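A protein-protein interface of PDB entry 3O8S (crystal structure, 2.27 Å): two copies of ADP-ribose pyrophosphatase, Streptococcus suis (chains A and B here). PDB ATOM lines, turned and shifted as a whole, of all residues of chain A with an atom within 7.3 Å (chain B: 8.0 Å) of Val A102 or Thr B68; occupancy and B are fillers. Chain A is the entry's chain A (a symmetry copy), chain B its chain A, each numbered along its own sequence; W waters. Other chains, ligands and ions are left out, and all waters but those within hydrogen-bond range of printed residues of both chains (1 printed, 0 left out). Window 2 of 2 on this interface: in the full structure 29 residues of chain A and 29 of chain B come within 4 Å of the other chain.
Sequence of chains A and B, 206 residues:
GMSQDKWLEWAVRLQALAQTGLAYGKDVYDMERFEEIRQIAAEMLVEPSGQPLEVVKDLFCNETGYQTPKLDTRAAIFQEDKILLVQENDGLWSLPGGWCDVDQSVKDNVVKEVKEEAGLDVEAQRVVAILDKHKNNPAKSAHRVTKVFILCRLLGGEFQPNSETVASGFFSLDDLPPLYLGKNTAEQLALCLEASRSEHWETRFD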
ATOM      1  N   THR A  68     -26.094   6.744 -17.753  1.00  0.00           N
ATOM      2  CA  THR A  68     -27.021   6.224 -18.757  1.00  0.00           C
ATOM      3  C   THR A  68     -26.301   6.053 -20.123  1.00  0.00           C
ATOM      4  O   THR A  68     -25.175   6.549 -20.255  1.00  0.00           O
ATOM      5  CB  THR A  68     -28.273   7.139 -18.880  1.00  0.00           C
ATOM      6  OG1 THR A  68     -27.931   8.373 -19.510  1.00  0.00           O
ATOM      7  CG2 THR A  68     -28.981   7.374 -17.558  1.00  0.00           C
ATOM      8  N   PRO A  69     -26.906   5.386 -21.155  1.00  0.00           N
ATOM      9  CA  PRO A  69     -26.220   5.280 -22.457  1.00  0.00           C
ATOM     10  C   PRO A  69     -26.111   6.628 -23.172  1.00  0.00           C
ATOM     11  O   PRO A  69     -27.039   7.449 -23.083  1.00  0.00           O
ATOM     12  CB  PRO A  69     -27.113   4.322 -23.266  1.00  0.00           C
ATOM     13  CG  PRO A  69     -28.048   3.704 -22.281  1.00  0.00           C
ATOM     14  CD  PRO A  69     -28.225   4.721 -21.205  1.00  0.00           C
ATOM     15  N   LYS A  70     -24.974   6.854 -23.873  1.00  0.00           N
ATOM     16  CA  LYS A  70     -24.736   8.068 -24.659  1.00  0.00           C
ATOM     17  C   LYS A  70     -25.767   8.146 -25.791  1.00  0.00           C
ATOM     18  O   LYS A  70     -26.100   7.117 -26.383  1.00  0.00           O
ATOM     19  CB  LYS A  70     -23.300   8.099 -25.218  1.00  0.00           C
ATOM     20  CG  LYS A  70     -22.250   8.477 -24.185  1.00  0.00           C
ATOM     21  N   LEU A  71     -26.326   9.343 -26.030  1.00  0.00           N
ATOM     22  CA  LEU A  71     -27.342   9.562 -27.057  1.00  0.00           C
ATOM     23  C   LEU A  71     -26.718  10.014 -28.367  1.00  0.00           C
ATOM     24  O   LEU A  71     -25.962  10.982 -28.383  1.00  0.00           O
ATOM     25  CB  LEU A  71     -28.360  10.626 -26.601  1.00  0.00           C
ATOM     26  CG  LEU A  71     -29.795  10.199 -26.251  1.00  0.00           C
ATOM     27  CD1 LEU A  71     -30.679  11.413 -26.092  1.00  0.00           C
ATOM     28  CD2 LEU A  71     -30.412   9.320 -27.317  1.00  0.00           C
ATOM     29  N   ASP A  72     -27.062   9.335 -29.469  1.00  0.00           N
ATOM     30  CA  ASP A  72     -26.618   9.679 -30.814  1.00  0.00           C
ATOM     31  C   ASP A  72     -27.839  10.014 -31.665  1.00  0.00           C
ATOM     32  O   ASP A  72     -28.835   9.294 -31.618  1.00  0.00           O
ATOM     33  CB  ASP A  72     -25.810   8.537 -31.445  1.00  0.00           C
ATOM     34  CG  ASP A  72     -25.333   8.825 -32.858  1.00  0.00           C
ATOM     35  OD1 ASP A  72     -24.462   9.693 -33.019  1.00  0.00           O
ATOM     36  OD2 ASP A  72     -25.819   8.160 -33.795  1.00  0.00           O
ATOM     37  N   GLY A  98     -24.642  12.957 -34.767  1.00  0.00           N
ATOM     38  CA  GLY A  98     -23.631  12.875 -33.731  1.00  0.00           C
ATOM     39  C   GLY A  98     -24.253  12.853 -32.361  1.00  0.00           C
ATOM     40  O   GLY A  98     -25.482  12.778 -32.215  1.00  0.00           O
ATOM     41  N   TRP A  99     -23.398  12.898 -31.352  1.00  0.00           N
ATOM     42  CA  TRP A  99     -23.809  12.850 -29.960  1.00  0.00           C
ATOM     43  C   TRP A  99     -24.553  14.103 -29.582  1.00  0.00           C
ATOM     44  O   TRP A  99     -24.176  15.213 -29.968  1.00  0.00           O
ATOM     45  CB  TRP A  99     -22.620  12.594 -29.043  1.00  0.00           C
ATOM     46  CG  TRP A  99     -22.134  11.178 -29.122  1.00  0.00           C
ATOM     47  CD1 TRP A  99     -22.849  10.046 -28.855  1.00  0.00           C
ATOM     48  CD2 TRP A  99     -20.816  10.746 -29.480  1.00  0.00           C
ATOM     49  NE1 TRP A  99     -22.059   8.935 -29.029  1.00  0.00           N
ATOM     50  CE2 TRP A  99     -20.802   9.334 -29.402  1.00  0.00           C
ATOM     51  CE3 TRP A  99     -19.642  11.418 -29.870  1.00  0.00           C
ATOM     52  CZ2 TRP A  99     -19.659   8.578 -29.695  1.00  0.00           C
ATOM     53  CZ3 TRP A  99     -18.509  10.670 -30.161  1.00  0.00           C
ATOM     54  CH2 TRP A  99     -18.521   9.268 -30.063  1.00  0.00           C
ATOM     55  N   CYS A 100     -25.663  13.893 -28.889  1.00  0.00           N
ATOM     56  CA  CYS A 100     -26.588  14.923 -28.483  1.00  0.00           C
ATOM     57  C   CYS A 100     -25.962  15.835 -27.448  1.00  0.00           C
ATOM     58  O   CYS A 100     -25.510  15.373 -26.401  1.00  0.00           O
ATOM     59  CB  CYS A 100     -27.886  14.301 -27.974  1.00  0.00           C
ATOM     60  SG  CYS A 100     -29.224  15.490 -27.709  1.00  0.00           S
ATOM     61  N   ASP A 101     -25.907  17.138 -27.769  1.00  0.00           N
ATOM     62  CA  ASP A 101     -25.413  18.191 -26.883  1.00  0.00           C
ATOM     63  C   ASP A 101     -26.203  18.114 -25.576  1.00  0.00           C
ATOM     64  O   ASP A 101     -27.427  17.934 -25.607  1.00  0.00           O
ATOM     65  CB  ASP A 101     -25.575  19.560 -27.560  1.00  0.00           C
ATOM     66  CG  ASP A 101     -24.688  20.631 -26.986  1.00  0.00           C
ATOM     67  OD1 ASP A 101     -25.035  21.178 -25.916  1.00  0.00           O
ATOM     68  OD2 ASP A 101     -23.658  20.941 -27.616  1.00  0.00           O
ATOM     69  N   VAL A 102     -25.497  18.161 -24.440  1.00  0.00           N
ATOM     70  CA  VAL A 102     -26.064  18.013 -23.094  1.00  0.00           C
ATOM     71  C   VAL A 102     -27.211  19.009 -22.839  1.00  0.00           C
ATOM     72  O   VAL A 102     -28.222  18.611 -22.267  1.00  0.00           O
ATOM     73  CB  VAL A 102     -24.988  18.113 -21.973  1.00  0.00           C
ATOM     74  CG1 VAL A 102     -25.456  17.405 -20.705  1.00  0.00           C
ATOM     75  CG2 VAL A 102     -23.642  17.549 -22.427  1.00  0.00           C
ATOM     76  N   ASP A 103     -27.076  20.264 -23.284  1.00  0.00           N
ATOM     77  CA  ASP A 103     -28.074  21.310 -23.050  1.00  0.00           C
ATOM     78  C   ASP A 103     -29.122  21.413 -24.162  1.00  0.00           C
ATOM     79  O   ASP A 103     -29.985  22.289 -24.093  1.00  0.00           O
ATOM     80  CB  ASP A 103     -27.375  22.673 -22.849  1.00  0.00           C
ATOM     81  CG  ASP A 103     -26.466  22.748 -21.632  1.00  0.00           C
ATOM     82  OD1 ASP A 103     -26.359  21.734 -20.903  1.00  0.00           O
ATOM     83  OD2 ASP A 103     -25.859  23.819 -21.411  1.00  0.00           O
ATOM     84  N   GLN A 104     -29.083  20.514 -25.158  1.00  0.00           N
ATOM     85  CA  GLN A 104     -30.052  20.563 -26.246  1.00  0.00           C
ATOM     86  C   GLN A 104     -30.902  19.315 -26.316  1.00  0.00           C
ATOM     87  O   GLN A 104     -30.449  18.224 -25.963  1.00  0.00           O
ATOM     88  CB  GLN A 104     -29.352  20.803 -27.586  1.00  0.00           C
ATOM     89  CG  GLN A 104     -29.008  22.275 -27.784  1.00  0.00           C
ATOM     90  CD  GLN A 104     -28.224  22.513 -29.037  1.00  0.00           C
ATOM     91  OE1 GLN A 104     -28.785  22.774 -30.107  1.00  0.00           O
ATOM     92  NE2 GLN A 104     -26.904  22.472 -28.920  1.00  0.00           N
ATOM     93  N   SER A 105     -32.146  19.492 -26.781  1.00  0.00           N
ATOM     94  CA  SER A 105     -33.110  18.427 -27.015  1.00  0.00           C
ATOM     95  C   SER A 105     -32.722  17.658 -28.289  1.00  0.00           C
ATOM     96  O   SER A 105     -31.930  18.165 -29.087  1.00  0.00           O
ATOM     97  CB  SER A 105     -34.514  19.013 -27.158  1.00  0.00           C
ATOM     98  OG  SER A 105     -34.691  19.635 -28.424  1.00  0.00           O
ATOM     99  N   ASN A 109     -30.915  19.424 -31.491  1.00  0.00           N
ATOM    100  CA  ASN A 109     -29.615  18.850 -31.777  1.00  0.00           C
ATOM    101  C   ASN A 109     -29.497  18.370 -33.251  1.00  0.00           C
ATOM    102  O   ASN A 109     -28.517  18.742 -33.893  1.00  0.00           O
ATOM    103  CB  ASN A 109     -29.315  17.718 -30.805  1.00  0.00           C
ATOM    104  CG  ASN A 109     -27.878  17.326 -30.789  1.00  0.00           C
ATOM    105  OD1 ASN A 109     -27.035  17.977 -30.169  1.00  0.00           O
ATOM    106  ND2 ASN A 109     -27.571  16.249 -31.478  1.00  0.00           N
ATOM    107  N   THR B  68     -23.661  13.608 -23.110  1.00  0.00           N
ATOM    108  CA  THR B  68     -24.995  13.685 -23.703  1.00  0.00           C
ATOM    109  C   THR B  68     -26.077  13.785 -22.591  1.00  0.00           C
ATOM    110  O   THR B  68     -25.732  13.578 -21.422  1.00  0.00           O
ATOM    111  CB  THR B  68     -25.252  12.474 -24.645  1.00  0.00           C
ATOM    112  OG1 THR B  68     -25.413  11.276 -23.887  1.00  0.00           O
ATOM    113  CG2 THR B  68     -24.192  12.307 -25.717  1.00  0.00           C
ATOM    114  N   PRO B  69     -27.378  14.077 -22.905  1.00  0.00           N
ATOM    115  CA  PRO B  69     -28.394  14.119 -21.835  1.00  0.00           C
ATOM    116  C   PRO B  69     -28.673  12.737 -21.241  1.00  0.00           C
ATOM    117  O   PRO B  69     -28.662  11.736 -21.976  1.00  0.00           O
ATOM    118  CB  PRO B  69     -29.651  14.655 -22.543  1.00  0.00           C
ATOM    119  CG  PRO B  69     -29.186  15.181 -23.860  1.00  0.00           C
ATOM    120  CD  PRO B  69     -27.991  14.364 -24.218  1.00  0.00           C
ATOM    121  N   LYS B  70     -28.917  12.687 -19.908  1.00  0.00           N
ATOM    122  CA  LYS B  70     -29.257  11.453 -19.194  1.00  0.00           C
ATOM    123  C   LYS B  70     -30.587  10.911 -19.729  1.00  0.00           C
ATOM    124  O   LYS B  70     -31.495  11.696 -20.012  1.00  0.00           O
ATOM    125  CB  LYS B  70     -29.329  11.690 -17.673  1.00  0.00           C
ATOM    126  CG  LYS B  70     -27.967  11.784 -17.004  1.00  0.00           C
ATOM    127  N   LEU B  71     -30.669   9.588 -19.943  1.00  0.00           N
ATOM    128  CA  LEU B  71     -31.863   8.935 -20.474  1.00  0.00           C
ATOM    129  C   LEU B  71     -32.763   8.429 -19.359  1.00  0.00           C
ATOM    130  O   LEU B  71     -32.302   7.701 -18.485  1.00  0.00           O
ATOM    131  CB  LEU B  71     -31.480   7.746 -21.379  1.00  0.00           C
ATOM    132  CG  LEU B  71     -31.701   7.849 -22.897  1.00  0.00           C
ATOM    133  CD1 LEU B  71     -31.510   6.499 -23.547  1.00  0.00           C
ATOM    134  CD2 LEU B  71     -33.090   8.334 -23.248  1.00  0.00           C
ATOM    135  N   ASP B 132     -37.863  16.187 -23.919  1.00  0.00           N
ATOM    136  CA  ASP B 132     -36.892  16.915 -23.150  1.00  0.00           C
ATOM    137  C   ASP B 132     -37.551  17.346 -21.831  1.00  0.00           C
ATOM    138  O   ASP B 132     -38.542  18.084 -21.862  1.00  0.00           O
ATOM    139  CB  ASP B 132     -36.404  18.105 -23.975  1.00  0.00           C
ATOM    140  CG  ASP B 132     -35.422  18.971 -23.253  1.00  0.00           C
ATOM    141  OD1 ASP B 132     -34.277  18.521 -23.043  1.00  0.00           O
ATOM    142  OD2 ASP B 132     -35.796  20.093 -22.885  1.00  0.00           O
ATOM    143  N   ARG B 144     -30.734  18.057 -17.281  1.00  0.00           N
ATOM    144  CA  ARG B 144     -30.656  17.763 -18.717  1.00  0.00           C
ATOM    145  C   ARG B 144     -31.024  16.287 -18.946  1.00  0.00           C
ATOM    146  O   ARG B 144     -30.166  15.398 -18.910  1.00  0.00           O
ATOM    147  CB  ARG B 144     -29.254  18.098 -19.252  1.00  0.00           C
ATOM    148  N   VAL B 145     -32.326  16.023 -19.088  1.00  0.00           N
ATOM    149  CA  VAL B 145     -32.835  14.654 -19.197  1.00  0.00           C
ATOM    150  C   VAL B 145     -33.722  14.506 -20.439  1.00  0.00           C
ATOM    151  O   VAL B 145     -34.564  15.367 -20.711  1.00  0.00           O
ATOM    152  CB  VAL B 145     -33.600  14.241 -17.888  1.00  0.00           C
ATOM    153  CG1 VAL B 145     -34.134  12.814 -17.962  1.00  0.00           C
ATOM    154  CG2 VAL B 145     -32.738  14.418 -16.629  1.00  0.00           C
ATOM    155  N   THR B 146     -33.526  13.405 -21.184  1.00  0.00           N
ATOM    156  CA  THR B 146     -34.361  13.027 -22.312  1.00  0.00           C
ATOM    157  C   THR B 146     -35.243  11.906 -21.750  1.00  0.00           C
ATOM    158  O   THR B 146     -34.725  10.927 -21.188  1.00  0.00           O
ATOM    159  CB  THR B 146     -33.509  12.668 -23.543  1.00  0.00           C
ATOM    160  OG1 THR B 146     -33.030  13.876 -24.142  1.00  0.00           O
ATOM    161  CG2 THR B 146     -34.295  11.862 -24.595  1.00  0.00           C
HETATM  162  O   HOH W   1     -31.871  19.738 -22.712  1.00  0.00           O
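OG1 of Thr B68 sits at hydrogen-bond distance from N of Leu A71 (3.0 Å). N of Leu B71 lies within hydrogen-bond range of OG1 of Thr A68.
The backbone carbonyl oxygen (O) of Arg B144 is in hydrogen-bond range of the backbone NH (N) of Lys B70. The side-chain sulfur (SG) of Cys A100 sits at hydrogen-bond distance from the backbone carbonyl oxygen (O) of Gln A104. The backbone NH (N) of Cys A100 is in hydrogen-bond range of the backbone carbonyl oxygen (O) of Leu A71. The backbone NH (N) of Asp A101 sits at hydrogen-bond distance from the side-chain amide oxygen (OD1) of Asn A109 (2.8 Å). N of Asp A103 sits close to OD1 of Asp A101. N of Thr B146 sits at hydrogen-bond distance from O of Lys B70, 2.9 Å away.
Among the printed residues, merely in contact across the chains: Thr A68 with Lys B70, Lys A70 with Thr B68, Leu A71 with Thr B146, Trp A99 with Thr B68, Cys A100 with Thr B68, Cys A100 with Pro B69, Asp A101 with Pro B69, Val A102 with Thr B68, Val A102 with Pro B69, Val A102 with Arg B144, Gln A104 with Pro B69 and Ser A105 with Asp B132.
Of the printed residues of chain B, Val A102 touches Thr B68, Pro B69 and Arg B144. Printed residues of chain A within 4 Å of Thr B68: Lys A70 (3.4 Å), Leu A71 (3.0 Å), Trp A99 (3.7 Å), Cys A100 (3.2 Å) and Val A102 (3.9 Å). Printed residues of chain A within 4 Å of Pro B69: Cys A100 (3.5 Å), Asp A101 (3.7 Å), Val A102 (3.9 Å) and Gln A104 (3.9 Å). Printed residues of chain A within 4 Å of Asp B132: Ser A105 (3.8 Å). Of the printed residues of chain A, Arg B144 touches Val A102. Val B145 touches none of the printed residues of chain A. The nearest residue of chain B that does not touch Val A102 is Val B145 (5.8 Å). The nearest residue of chain A that does not touch Thr B68 is Pro A69 (4.2 Å). The nearest printed residue of chain B that does not touch Trp A99 is Pro B69 (6.4 Å).
Of the 8 printed residues of chain B, 7 touch a printed residue of chain A. Printed residues of chain B that touch a printed residue of chain A: Thr B68, Pro B69, Lys B70, Leu B71, Asp B132, Arg B144 and Thr B146. Among the printed residues, 14 pairs touch across the chains. Among the printed residues, no Asp or Glu carboxylate lies within 4 Å of a Lys or Arg side-chain nitrogen of the other chain.
Thr A68 touches Lys B70, and with the chains exchanged Lys A70 touches Thr B68. Thr A68 touches Leu B71, and with the chains exchanged Leu A71 touches Thr B68. Of the 14 pairs that touch across the chains among the printed residues, 4 have their exchanged pair printed and touching as well.
Water W1 bridges OD1 of Asp B132 (2.7 Å) and O of Asp A103 (3.5 Å).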
